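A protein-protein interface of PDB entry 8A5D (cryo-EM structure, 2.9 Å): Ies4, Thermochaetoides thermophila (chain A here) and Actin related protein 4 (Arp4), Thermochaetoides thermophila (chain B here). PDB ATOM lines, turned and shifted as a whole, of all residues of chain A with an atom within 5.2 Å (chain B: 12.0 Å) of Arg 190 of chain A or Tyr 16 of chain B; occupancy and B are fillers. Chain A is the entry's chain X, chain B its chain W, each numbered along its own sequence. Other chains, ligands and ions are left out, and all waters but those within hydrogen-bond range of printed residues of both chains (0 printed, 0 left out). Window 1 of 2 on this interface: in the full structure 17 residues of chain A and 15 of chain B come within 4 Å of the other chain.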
ATOM      1  N   TRP A 171     -20.704 -19.848  -7.049  1.00  0.00           N
ATOM      2  CA  TRP A 171     -20.011 -19.686  -8.337  1.00  0.00           C
ATOM      3  C   TRP A 171     -20.974 -19.252  -9.448  1.00  0.00           C
ATOM      4  O   TRP A 171     -22.112 -19.702  -9.473  1.00  0.00           O
ATOM      5  CB  TRP A 171     -19.329 -21.006  -8.663  1.00  0.00           C
ATOM      6  CG  TRP A 171     -18.161 -21.307  -7.797  1.00  0.00           C
ATOM      7  CD1 TRP A 171     -18.185 -21.944  -6.611  1.00  0.00           C
ATOM      8  CD2 TRP A 171     -16.790 -20.958  -8.043  1.00  0.00           C
ATOM      9  NE1 TRP A 171     -16.920 -22.047  -6.091  1.00  0.00           N
ATOM     10  CE2 TRP A 171     -16.037 -21.451  -6.942  1.00  0.00           C
ATOM     11  CE3 TRP A 171     -16.137 -20.256  -9.077  1.00  0.00           C
ATOM     12  CZ2 TRP A 171     -14.647 -21.370  -6.881  1.00  0.00           C
ATOM     13  CZ3 TRP A 171     -14.776 -20.102  -8.992  1.00  0.00           C
ATOM     14  CH2 TRP A 171     -14.052 -20.658  -7.906  1.00  0.00           C
ATOM     15  N   THR A 172     -20.518 -18.428 -10.379  1.00  0.00           N
ATOM     16  CA  THR A 172     -21.364 -17.778 -11.411  1.00  0.00           C
ATOM     17  C   THR A 172     -20.556 -17.670 -12.707  1.00  0.00           C
ATOM     18  O   THR A 172     -19.340 -17.330 -12.604  1.00  0.00           O
ATOM     19  CB  THR A 172     -21.780 -16.356 -10.983  1.00  0.00           C
ATOM     20  OG1 THR A 172     -22.242 -16.323  -9.623  1.00  0.00           O
ATOM     21  CG2 THR A 172     -22.780 -15.752 -11.954  1.00  0.00           C
ATOM     22  N   ARG A 173     -21.192 -17.855 -13.878  1.00  0.00           N
ATOM     23  CA  ARG A 173     -20.521 -17.674 -15.196  1.00  0.00           C
ATOM     24  C   ARG A 173     -20.247 -16.189 -15.397  1.00  0.00           C
ATOM     25  O   ARG A 173     -21.218 -15.442 -15.609  1.00  0.00           O
ATOM     26  CB  ARG A 173     -21.332 -18.241 -16.365  1.00  0.00           C
ATOM     27  CG  ARG A 173     -21.544 -19.755 -16.348  1.00  0.00           C
ATOM     28  CD  ARG A 173     -20.300 -20.641 -16.383  1.00  0.00           C
ATOM     29  NE  ARG A 173     -19.711 -20.747 -17.711  1.00  0.00           N
ATOM     30  CZ  ARG A 173     -18.482 -21.204 -17.961  1.00  0.00           C
ATOM     31  NH1 ARG A 173     -17.681 -21.555 -16.969  1.00  0.00           N
ATOM     32  NH2 ARG A 173     -18.036 -21.276 -19.206  1.00  0.00           N
ATOM     33  N   GLY A 174     -18.976 -15.785 -15.253  1.00  0.00           N
ATOM     34  CA  GLY A 174     -18.451 -14.444 -15.591  1.00  0.00           C
ATOM     35  C   GLY A 174     -17.713 -14.445 -16.913  1.00  0.00           C
ATOM     36  O   GLY A 174     -17.887 -15.371 -17.735  1.00  0.00           O
ATOM     37  N   THR A 175     -16.912 -13.411 -17.132  1.00  0.00           N
ATOM     38  CA  THR A 175     -16.086 -13.224 -18.353  1.00  0.00           C
ATOM     39  C   THR A 175     -14.676 -12.822 -17.936  1.00  0.00           C
ATOM     40  O   THR A 175     -14.503 -12.061 -16.950  1.00  0.00           O
ATOM     41  CB  THR A 175     -16.676 -12.187 -19.316  1.00  0.00           C
ATOM     42  OG1 THR A 175     -16.974 -10.972 -18.617  1.00  0.00           O
ATOM     43  CG2 THR A 175     -17.916 -12.715 -20.004  1.00  0.00           C
ATOM     44  N   PHE A 176     -13.703 -13.339 -18.674  1.00  0.00           N
ATOM     45  CA  PHE A 176     -12.263 -13.169 -18.391  1.00  0.00           C
ATOM     46  C   PHE A 176     -11.627 -12.568 -19.631  1.00  0.00           C
ATOM     47  O   PHE A 176     -11.767 -13.152 -20.722  1.00  0.00           O
ATOM     48  CB  PHE A 176     -11.658 -14.507 -18.048  1.00  0.00           C
ATOM     49  CG  PHE A 176     -10.206 -14.465 -17.688  1.00  0.00           C
ATOM     50  CD1 PHE A 176      -9.772 -13.712 -16.617  1.00  0.00           C
ATOM     51  CD2 PHE A 176      -9.300 -15.270 -18.352  1.00  0.00           C
ATOM     52  CE1 PHE A 176      -8.443 -13.724 -16.246  1.00  0.00           C
ATOM     53  CE2 PHE A 176      -7.971 -15.288 -17.972  1.00  0.00           C
ATOM     54  CZ  PHE A 176      -7.545 -14.510 -16.926  1.00  0.00           C
ATOM     55  N   ILE A 188     -13.305 -14.667 -22.816  1.00  0.00           N
ATOM     56  CA  ILE A 188     -13.718 -16.087 -22.679  1.00  0.00           C
ATOM     57  C   ILE A 188     -14.650 -16.193 -21.468  1.00  0.00           C
ATOM     58  O   ILE A 188     -14.409 -15.591 -20.419  1.00  0.00           O
ATOM     59  CB  ILE A 188     -12.483 -17.016 -22.590  1.00  0.00           C
ATOM     60  CG1 ILE A 188     -12.882 -18.459 -22.866  1.00  0.00           C
ATOM     61  CG2 ILE A 188     -11.719 -16.913 -21.268  1.00  0.00           C
ATOM     62  CD1 ILE A 188     -13.209 -18.711 -24.320  1.00  0.00           C
ATOM     63  N   PRO A 189     -15.802 -16.899 -21.584  1.00  0.00           N
ATOM     64  CA  PRO A 189     -16.638 -17.184 -20.418  1.00  0.00           C
ATOM     65  C   PRO A 189     -15.925 -18.074 -19.408  1.00  0.00           C
ATOM     66  O   PRO A 189     -15.251 -18.995 -19.822  1.00  0.00           O
ATOM     67  CB  PRO A 189     -17.842 -17.885 -21.046  1.00  0.00           C
ATOM     68  CG  PRO A 189     -17.908 -17.252 -22.407  1.00  0.00           C
ATOM     69  CD  PRO A 189     -16.461 -17.312 -22.832  1.00  0.00           C
ATOM     70  N   ARG A 190     -16.129 -17.819 -18.137  1.00  0.00           N
ATOM     71  CA  ARG A 190     -15.343 -18.487 -17.081  1.00  0.00           C
ATOM     72  C   ARG A 190     -16.100 -18.509 -15.744  1.00  0.00           C
ATOM     73  O   ARG A 190     -16.846 -17.586 -15.444  1.00  0.00           O
ATOM     74  CB  ARG A 190     -14.018 -17.738 -16.983  1.00  0.00           C
ATOM     75  CG  ARG A 190     -12.975 -18.443 -16.142  1.00  0.00           C
ATOM     76  CD  ARG A 190     -11.581 -17.849 -16.266  1.00  0.00           C
ATOM     77  NE  ARG A 190     -10.677 -18.723 -15.538  1.00  0.00           N
ATOM     78  CZ  ARG A 190      -9.471 -18.401 -15.125  1.00  0.00           C
ATOM     79  NH1 ARG A 190      -8.981 -17.190 -15.354  1.00  0.00           N
ATOM     80  NH2 ARG A 190      -8.769 -19.305 -14.461  1.00  0.00           N
ATOM     81  N   TRP A 191     -15.910 -19.524 -14.912  1.00  0.00           N
ATOM     82  CA  TRP A 191     -16.557 -19.548 -13.573  1.00  0.00           C
ATOM     83  C   TRP A 191     -15.839 -18.596 -12.643  1.00  0.00           C
ATOM     84  O   TRP A 191     -14.628 -18.652 -12.596  1.00  0.00           O
ATOM     85  CB  TRP A 191     -16.574 -20.926 -12.962  1.00  0.00           C
ATOM     86  CG  TRP A 191     -17.501 -21.914 -13.596  1.00  0.00           C
ATOM     87  CD1 TRP A 191     -17.156 -23.036 -14.290  1.00  0.00           C
ATOM     88  CD2 TRP A 191     -18.928 -21.954 -13.485  1.00  0.00           C
ATOM     89  NE1 TRP A 191     -18.271 -23.740 -14.655  1.00  0.00           N
ATOM     90  CE2 TRP A 191     -19.369 -23.127 -14.133  1.00  0.00           C
ATOM     91  CE3 TRP A 191     -19.871 -21.129 -12.887  1.00  0.00           C
ATOM     92  CZ2 TRP A 191     -20.716 -23.469 -14.226  1.00  0.00           C
ATOM     93  CZ3 TRP A 191     -21.203 -21.474 -12.945  1.00  0.00           C
ATOM     94  CH2 TRP A 191     -21.620 -22.618 -13.631  1.00  0.00           C
ATOM     95  N   THR A 192     -16.601 -17.793 -11.892  1.00  0.00           N
ATOM     96  CA  THR A 192     -16.101 -16.808 -10.894  1.00  0.00           C
ATOM     97  C   THR A 192     -16.855 -16.894  -9.574  1.00  0.00           C
ATOM     98  O   THR A 192     -18.033 -17.274  -9.573  1.00  0.00           O
ATOM     99  CB  THR A 192     -16.239 -15.394 -11.420  1.00  0.00           C
ATOM    100  OG1 THR A 192     -17.630 -15.111 -11.563  1.00  0.00           O
ATOM    101  CG2 THR A 192     -15.543 -15.246 -12.754  1.00  0.00           C
ATOM    102  N   ALA A 193     -16.158 -16.567  -8.494  1.00  0.00           N
ATOM    103  CA  ALA A 193     -16.695 -16.524  -7.123  1.00  0.00           C
ATOM    104  C   ALA A 193     -16.242 -15.244  -6.430  1.00  0.00           C
ATOM    105  O   ALA A 193     -15.183 -14.716  -6.742  1.00  0.00           O
ATOM    106  CB  ALA A 193     -16.242 -17.737  -6.402  1.00  0.00           C
ATOM    107  N   ALA B  13      -6.584 -11.005  -7.223  1.00  0.00           N
ATOM    108  CA  ALA B  13      -8.009 -11.295  -7.604  1.00  0.00           C
ATOM    109  C   ALA B  13      -8.607 -12.382  -6.690  1.00  0.00           C
ATOM    110  O   ALA B  13      -9.489 -12.038  -5.874  1.00  0.00           O
ATOM    111  CB  ALA B  13      -8.075 -11.691  -9.060  1.00  0.00           C
ATOM    112  N   ASP B  14      -8.165 -13.642  -6.846  1.00  0.00           N
ATOM    113  CA  ASP B  14      -8.602 -14.837  -6.062  1.00  0.00           C
ATOM    114  C   ASP B  14     -10.092 -15.139  -6.314  1.00  0.00           C
ATOM    115  O   ASP B  14     -10.716 -15.829  -5.469  1.00  0.00           O
ATOM    116  CB  ASP B  14      -8.295 -14.654  -4.569  1.00  0.00           C
ATOM    117  CG  ASP B  14      -8.234 -15.940  -3.757  1.00  0.00           C
ATOM    118  OD1 ASP B  14      -8.404 -15.857  -2.523  1.00  0.00           O
ATOM    119  OD2 ASP B  14      -8.007 -17.013  -4.356  1.00  0.00           O
ATOM    120  N   ILE B  15     -10.630 -14.701  -7.453  1.00  0.00           N
ATOM    121  CA  ILE B  15     -12.052 -14.927  -7.813  1.00  0.00           C
ATOM    122  C   ILE B  15     -12.215 -16.148  -8.732  1.00  0.00           C
ATOM    123  O   ILE B  15     -13.377 -16.464  -9.024  1.00  0.00           O
ATOM    124  CB  ILE B  15     -12.681 -13.688  -8.475  1.00  0.00           C
ATOM    125  CG1 ILE B  15     -11.972 -13.270  -9.770  1.00  0.00           C
ATOM    126  CG2 ILE B  15     -12.806 -12.552  -7.477  1.00  0.00           C
ATOM    127  CD1 ILE B  15     -12.696 -12.165 -10.532  1.00  0.00           C
ATOM    128  N   TYR B  16     -11.160 -16.793  -9.225  1.00  0.00           N
ATOM    129  CA  TYR B  16     -11.285 -17.770 -10.344  1.00  0.00           C
ATOM    130  C   TYR B  16     -11.051 -19.206  -9.878  1.00  0.00           C
ATOM    131  O   TYR B  16     -10.215 -19.439  -8.975  1.00  0.00           O
ATOM    132  CB  TYR B  16     -10.308 -17.427 -11.473  1.00  0.00           C
ATOM    133  CG  TYR B  16     -10.661 -16.160 -12.200  1.00  0.00           C
ATOM    134  CD1 TYR B  16     -11.800 -16.087 -12.970  1.00  0.00           C
ATOM    135  CD2 TYR B  16      -9.883 -15.030 -12.084  1.00  0.00           C
ATOM    136  CE1 TYR B  16     -12.163 -14.921 -13.624  1.00  0.00           C
ATOM    137  CE2 TYR B  16     -10.222 -13.859 -12.739  1.00  0.00           C
ATOM    138  CZ  TYR B  16     -11.374 -13.796 -13.501  1.00  0.00           C
ATOM    139  OH  TYR B  16     -11.712 -12.638 -14.141  1.00  0.00           O
ATOM    140  N   GLY B  17     -11.702 -20.148 -10.575  1.00  0.00           N
ATOM    141  CA  GLY B  17     -11.613 -21.599 -10.309  1.00  0.00           C
ATOM    142  C   GLY B  17     -10.529 -22.319 -11.091  1.00  0.00           C
ATOM    143  O   GLY B  17      -9.598 -21.677 -11.613  1.00  0.00           O
ATOM    144  N   GLY B  18     -10.632 -23.642 -11.149  1.00  0.00           N
ATOM    145  CA  GLY B  18      -9.757 -24.507 -11.959  1.00  0.00           C
ATOM    146  C   GLY B  18     -10.056 -24.384 -13.444  1.00  0.00           C
ATOM    147  O   GLY B  18      -9.220 -24.782 -14.243  1.00  0.00           O
ATOM    148  N   ASP B  19     -11.241 -23.899 -13.794  1.00  0.00           N
ATOM    149  CA  ASP B  19     -11.693 -23.564 -15.169  1.00  0.00           C
ATOM    150  C   ASP B  19     -10.680 -22.613 -15.811  1.00  0.00           C
ATOM    151  O   ASP B  19     -10.379 -21.558 -15.194  1.00  0.00           O
ATOM    152  CB  ASP B  19     -13.075 -22.889 -15.075  1.00  0.00           C
ATOM    153  CG  ASP B  19     -13.830 -22.718 -16.384  1.00  0.00           C
ATOM    154  OD1 ASP B  19     -13.400 -23.312 -17.400  1.00  0.00           O
ATOM    155  OD2 ASP B  19     -14.844 -21.994 -16.371  1.00  0.00           O
ATOM    156  N   GLU B  20     -10.219 -22.890 -17.028  1.00  0.00           N
ATOM    157  CA  GLU B  20      -9.380 -21.914 -17.778  1.00  0.00           C
ATOM    158  C   GLU B  20      -9.978 -21.766 -19.179  1.00  0.00           C
ATOM    159  O   GLU B  20     -10.842 -20.889 -19.365  1.00  0.00           O
ATOM    160  CB  GLU B  20      -7.915 -22.346 -17.751  1.00  0.00           C
ATOM    161  CG  GLU B  20      -7.255 -22.153 -16.388  1.00  0.00           C
ATOM    162  CD  GLU B  20      -5.949 -22.899 -16.127  1.00  0.00           C
ATOM    163  OE1 GLU B  20      -5.837 -24.078 -16.522  1.00  0.00           O
ATOM    164  OE2 GLU B  20      -5.044 -22.300 -15.511  1.00  0.00           O
ATOM    165  N   VAL B  21      -9.539 -22.575 -20.138  1.00  0.00           N
ATOM    166  CA  VAL B  21     -10.142 -22.589 -21.495  1.00  0.00           C
ATOM    167  C   VAL B  21     -10.512 -24.027 -21.866  1.00  0.00           C
ATOM    168  O   VAL B  21      -9.618 -24.903 -21.873  1.00  0.00           O
ATOM    169  CB  VAL B  21      -9.200 -21.956 -22.529  1.00  0.00           C
ATOM    170  CG1 VAL B  21      -9.819 -21.992 -23.925  1.00  0.00           C
ATOM    171  CG2 VAL B  21      -8.843 -20.534 -22.137  1.00  0.00           C
ATOM    172  N   SER B  22     -11.785 -24.235 -22.189  1.00  0.00           N
ATOM    173  CA  SER B  22     -12.290 -25.496 -22.775  1.00  0.00           C
ATOM    174  C   SER B  22     -12.258 -25.341 -24.302  1.00  0.00           C
ATOM    175  O   SER B  22     -13.170 -24.737 -24.897  1.00  0.00           O
ATOM    176  CB  SER B  22     -13.647 -25.860 -22.222  1.00  0.00           C
ATOM    177  OG  SER B  22     -14.577 -24.803 -22.397  1.00  0.00           O
ATOM    178  N   ALA B  23     -11.202 -25.835 -24.932  1.00  0.00           N
ATOM    179  CA  ALA B  23     -11.047 -25.715 -26.394  1.00  0.00           C
ATOM    180  C   ALA B  23     -11.647 -26.965 -27.035  1.00  0.00           C
ATOM    181  O   ALA B  23     -11.503 -28.083 -26.467  1.00  0.00           O
ATOM    182  CB  ALA B  23      -9.588 -25.531 -26.750  1.00  0.00           C
ATOM    183  N   LEU B 141     -21.242 -22.125 -30.382  1.00  0.00           N
ATOM    184  CA  LEU B 141     -19.916 -22.435 -29.771  1.00  0.00           C
ATOM    185  C   LEU B 141     -19.326 -21.239 -29.011  1.00  0.00           C
ATOM    186  O   LEU B 141     -18.090 -21.179 -28.872  1.00  0.00           O
ATOM    187  CB  LEU B 141     -18.934 -22.977 -30.825  1.00  0.00           C
ATOM    188  CG  LEU B 141     -19.335 -24.281 -31.514  1.00  0.00           C
ATOM    189  CD1 LEU B 141     -18.255 -24.733 -32.472  1.00  0.00           C
ATOM    190  CD2 LEU B 141     -19.662 -25.377 -30.514  1.00  0.00           C
ATOM    191  N   THR B 142     -20.146 -20.404 -28.389  1.00  0.00           N
ATOM    192  CA  THR B 142     -19.711 -19.117 -27.782  1.00  0.00           C
ATOM    193  C   THR B 142     -18.731 -19.292 -26.613  1.00  0.00           C
ATOM    194  O   THR B 142     -18.157 -18.260 -26.202  1.00  0.00           O
ATOM    195  CB  THR B 142     -20.907 -18.287 -27.311  1.00  0.00           C
ATOM    196  OG1 THR B 142     -21.759 -19.087 -26.497  1.00  0.00           O
ATOM    197  CG2 THR B 142     -21.679 -17.732 -28.476  1.00  0.00           C
ATOM    198  N   GLU B 143     -18.516 -20.499 -26.100  1.00  0.00           N
ATOM    199  CA  GLU B 143     -17.719 -20.690 -24.867  1.00  0.00           C
ATOM    200  C   GLU B 143     -16.391 -21.362 -25.185  1.00  0.00           C
ATOM    201  O   GLU B 143     -15.565 -21.434 -24.261  1.00  0.00           O
ATOM    202  CB  GLU B 143     -18.505 -21.485 -23.823  1.00  0.00           C
ATOM    203  CG  GLU B 143     -19.770 -20.763 -23.387  1.00  0.00           C
ATOM    204  CD  GLU B 143     -20.575 -21.424 -22.277  1.00  0.00           C
ATOM    205  OE1 GLU B 143     -21.743 -21.801 -22.533  1.00  0.00           O
ATOM    206  OE2 GLU B 143     -20.045 -21.541 -21.148  1.00  0.00           O
ATOM    207  N   ASN B 144     -16.209 -21.898 -26.392  1.00  0.00           N
ATOM    208  CA  ASN B 144     -15.102 -22.854 -26.706  1.00  0.00           C
ATOM    209  C   ASN B 144     -14.372 -22.394 -27.955  1.00  0.00           C
ATOM    210  O   ASN B 144     -14.970 -22.420 -29.022  1.00  0.00           O
ATOM    211  CB  ASN B 144     -15.648 -24.260 -26.938  1.00  0.00           C
ATOM    212  CG  ASN B 144     -16.542 -24.735 -25.803  1.00  0.00           C
ATOM    213  OD1 ASN B 144     -16.110 -24.949 -24.650  1.00  0.00           O
ATOM    214  ND2 ASN B 144     -17.815 -24.899 -26.134  1.00  0.00           N
ATOM    215  N   PRO B 145     -13.076 -21.992 -27.897  1.00  0.00           N
ATOM    216  CA  PRO B 145     -12.315 -21.761 -29.117  1.00  0.00           C
ATOM    217  C   PRO B 145     -11.974 -23.099 -29.816  1.00  0.00           C
ATOM    218  O   PRO B 145     -11.898 -24.146 -29.188  1.00  0.00           O
ATOM    219  CB  PRO B 145     -11.126 -21.000 -28.551  1.00  0.00           C
ATOM    220  CG  PRO B 145     -10.874 -21.614 -27.205  1.00  0.00           C
ATOM    221  CD  PRO B 145     -12.261 -21.802 -26.689  1.00  0.00           C
ATOM    222  N   PRO B 173     -15.387 -18.052 -30.269  1.00  0.00           N
ATOM    223  CA  PRO B 173     -14.692 -16.860 -29.814  1.00  0.00           C
ATOM    224  C   PRO B 173     -13.359 -16.640 -30.532  1.00  0.00           C
ATOM    225  O   PRO B 173     -12.981 -15.500 -30.670  1.00  0.00           O
ATOM    226  CB  PRO B 173     -14.462 -17.096 -28.305  1.00  0.00           C
ATOM    227  CG  PRO B 173     -14.483 -18.545 -28.134  1.00  0.00           C
ATOM    228  CD  PRO B 173     -15.447 -19.043 -29.201  1.00  0.00           C
ATOM    229  N   SER B 441      -4.071 -27.307 -24.438  1.00  0.00           N
ATOM    230  CA  SER B 441      -4.123 -27.332 -22.959  1.00  0.00           C
ATOM    231  C   SER B 441      -2.898 -26.660 -22.306  1.00  0.00           C
ATOM    232  O   SER B 441      -2.884 -26.574 -21.058  1.00  0.00           O
ATOM    233  CB  SER B 441      -4.276 -28.747 -22.500  1.00  0.00           C
ATOM    234  OG  SER B 441      -3.016 -29.391 -22.497  1.00  0.00           O
ATOM    235  N   LEU B 442      -1.940 -26.144 -23.094  1.00  0.00           N
ATOM    236  CA  LEU B 442      -0.730 -25.415 -22.603  1.00  0.00           C
ATOM    237  C   LEU B 442      -1.068 -23.945 -22.335  1.00  0.00           C
ATOM    238  O   LEU B 442      -1.712 -23.276 -23.182  1.00  0.00           O
ATOM    239  CB  LEU B 442       0.400 -25.483 -23.626  1.00  0.00           C
ATOM    240  CG  LEU B 442       0.825 -26.889 -23.987  1.00  0.00           C
ATOM    241  CD1 LEU B 442       2.003 -26.859 -24.926  1.00  0.00           C
ATOM    242  CD2 LEU B 442       1.135 -27.648 -22.710  1.00  0.00           C
ATOM    243  N   GLY B 443      -0.612 -23.438 -21.203  1.00  0.00           N
ATOM    244  CA  GLY B 443      -0.996 -22.082 -20.790  1.00  0.00           C
ATOM    245  C   GLY B 443      -0.373 -21.071 -21.706  1.00  0.00           C
ATOM    246  O   GLY B 443      -1.051 -20.084 -22.040  1.00  0.00           O
ATOM    247  N   HIS B 446      -2.225 -19.893 -25.101  1.00  0.00           N
ATOM    248  CA  HIS B 446      -3.497 -19.109 -25.194  1.00  0.00           C
ATOM    249  C   HIS B 446      -3.251 -17.701 -25.740  1.00  0.00           C
ATOM    250  O   HIS B 446      -4.248 -17.092 -26.122  1.00  0.00           O
ATOM    251  CB  HIS B 446      -4.300 -19.114 -23.874  1.00  0.00           C
ATOM    252  CG  HIS B 446      -4.672 -20.485 -23.381  1.00  0.00           C
ATOM    253  ND1 HIS B 446      -5.111 -21.474 -24.236  1.00  0.00           N
ATOM    254  CD2 HIS B 446      -4.660 -21.036 -22.143  1.00  0.00           C
ATOM    255  CE1 HIS B 446      -5.337 -22.571 -23.576  1.00  0.00           C
ATOM    256  NE2 HIS B 446      -5.066 -22.335 -22.274  1.00  0.00           N
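The backbone carbonyl oxygen (O) of Asp 19 of chain B sits at hydrogen-bond distance from the guanidinium group (NH2) of Arg 190 of chain A. O of Ile 15 of chain B sits at hydrogen-bond distance from N of Ala 193 of chain A (2.8 Å). The side-chain carboxylate of Asp 19 of chain B lies within hydrogen-bond range of the backbone NH of Trp 191 of chain A (3.1 Å). OD2 of Asp 19 of chain B lies within salt-bridge range of NH1 of Arg 173 of chain A (2.9 Å). NH2 of Arg 173 of chain A lies within salt-bridge range of OE2 of Glu 143 of chain B (2.8 Å).
The backbone carbonyl oxygen (O) of Thr 192 of chain A lies within hydrogen-bond range of the backbone NH (N) of Thr 172 of chain A. N of Gly 174 of chain A sits at hydrogen-bond distance from O of Arg 190 of chain A, 2.8 Å away. N of Phe 176 of chain A sits at hydrogen-bond distance from O of Ile 188 of chain A (2.9 Å).
Trp 171 of chain A touches Ile 15 of chain B (CZ3 to O, 3.9 Å). C of Tyr 16 of chain B touches CH2 of Trp 171 of chain A, at 3.9 Å. Gly 17 of chain B touches Trp 171 of chain A. Phe 176 of chain A touches Tyr 16 of chain B (CD1 to OH, 3.3 Å). Glu 143 of chain B touches Ile 188 of chain A. Thr 142 of chain B touches Pro 189 of chain A (O to CD, 3.9 Å). Tyr 16 of chain B touches Arg 190 of chain A. O of Gly 17 of chain B touches NH2 of Arg 190 of chain A (3.8 Å). Glu 20 of chain B touches Arg 190 of chain A. Thr 192 of chain A touches Tyr 16 of chain B.
Of the printed residues of chain B, Trp 171 of chain A touches Ile 15 (3.9 Å), Tyr 16 (3.9 Å) and Gly 17 (3.5 Å). Of chain B, only Asp 19 and Glu 143 come within 4 Å of Arg 173 of chain A. No residue of chain B comes within 4 Å of Gly 174 of chain A. Printed residues of chain B within 4 Å of Ile 188 of chain A: Glu 143 (3.6 Å). Of chain B, only Thr 142 comes within 4 Å of Pro 189 of chain A. Arg 190 of chain A touches four residues of chain B. Of the printed residues of chain B, Trp 191 of chain A touches Tyr 16, Gly 17 and Asp 19. Thr 192 of chain A touches just these residues of chain B: Ile 15 (3.3 Å) and Tyr 16 (3.5 Å). Of chain B, only Ile 15 comes within 4 Å of Ala 193 of chain A. Printed residues of chain A within 4 Å of Tyr 16 of chain B: Trp 171 (3.9 Å), Phe 176 (3.3 Å), Arg 190 (3.7 Å), Trp 191 (3.8 Å) and Thr 192 (3.5 Å). Printed residues of chain A within 4 Å of Asp 19 of chain B: Arg 173, Arg 190 and Trp 191. Printed residues of chain A within 4 Å of Glu 20 of chain B: Arg 190. Ser 22 of chain B touches none of the printed residues of chain A. Printed residues of chain A within 4 Å of Thr 142 of chain B: Pro 189. The nearest residue of chain B that does not touch Arg 190 of chain A is Gly 18 of chain B (5.3 Å). The nearest printed residue of chain A that does not touch Gly 17 of chain B is Thr 192 of chain A (5.5 Å).
Of the 12 printed residues of chain A, 9 touch a printed residue of chain B. Hydrophobic or aromatic side chains of chain A within 4 Å of the printed part of chain B: Trp 171, Phe 176, Ile 188, Pro 189 and Trp 191. Along chain A the printed residues that touch a printed residue of chain B span positions 171 to 193. Printed residues of chain B that touch a printed residue of chain A: Ile 15, Tyr 16, Gly 17, Asp 19, Glu 20, Thr 142 and Glu 143. Hydrophobic or aromatic side chains of chain B within 4 Å of the printed part of chain A: Ile 15 and Tyr 16. Among the printed residues, Asp or Glu carboxylates within 4 Å of a Lys or Arg side-chain nitrogen of the other chain: Arg 173 of chain A with Asp 19 of chain B (2.9 Å) and Arg 173 of chain A with Glu 143 of chain B (2.8 Å).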
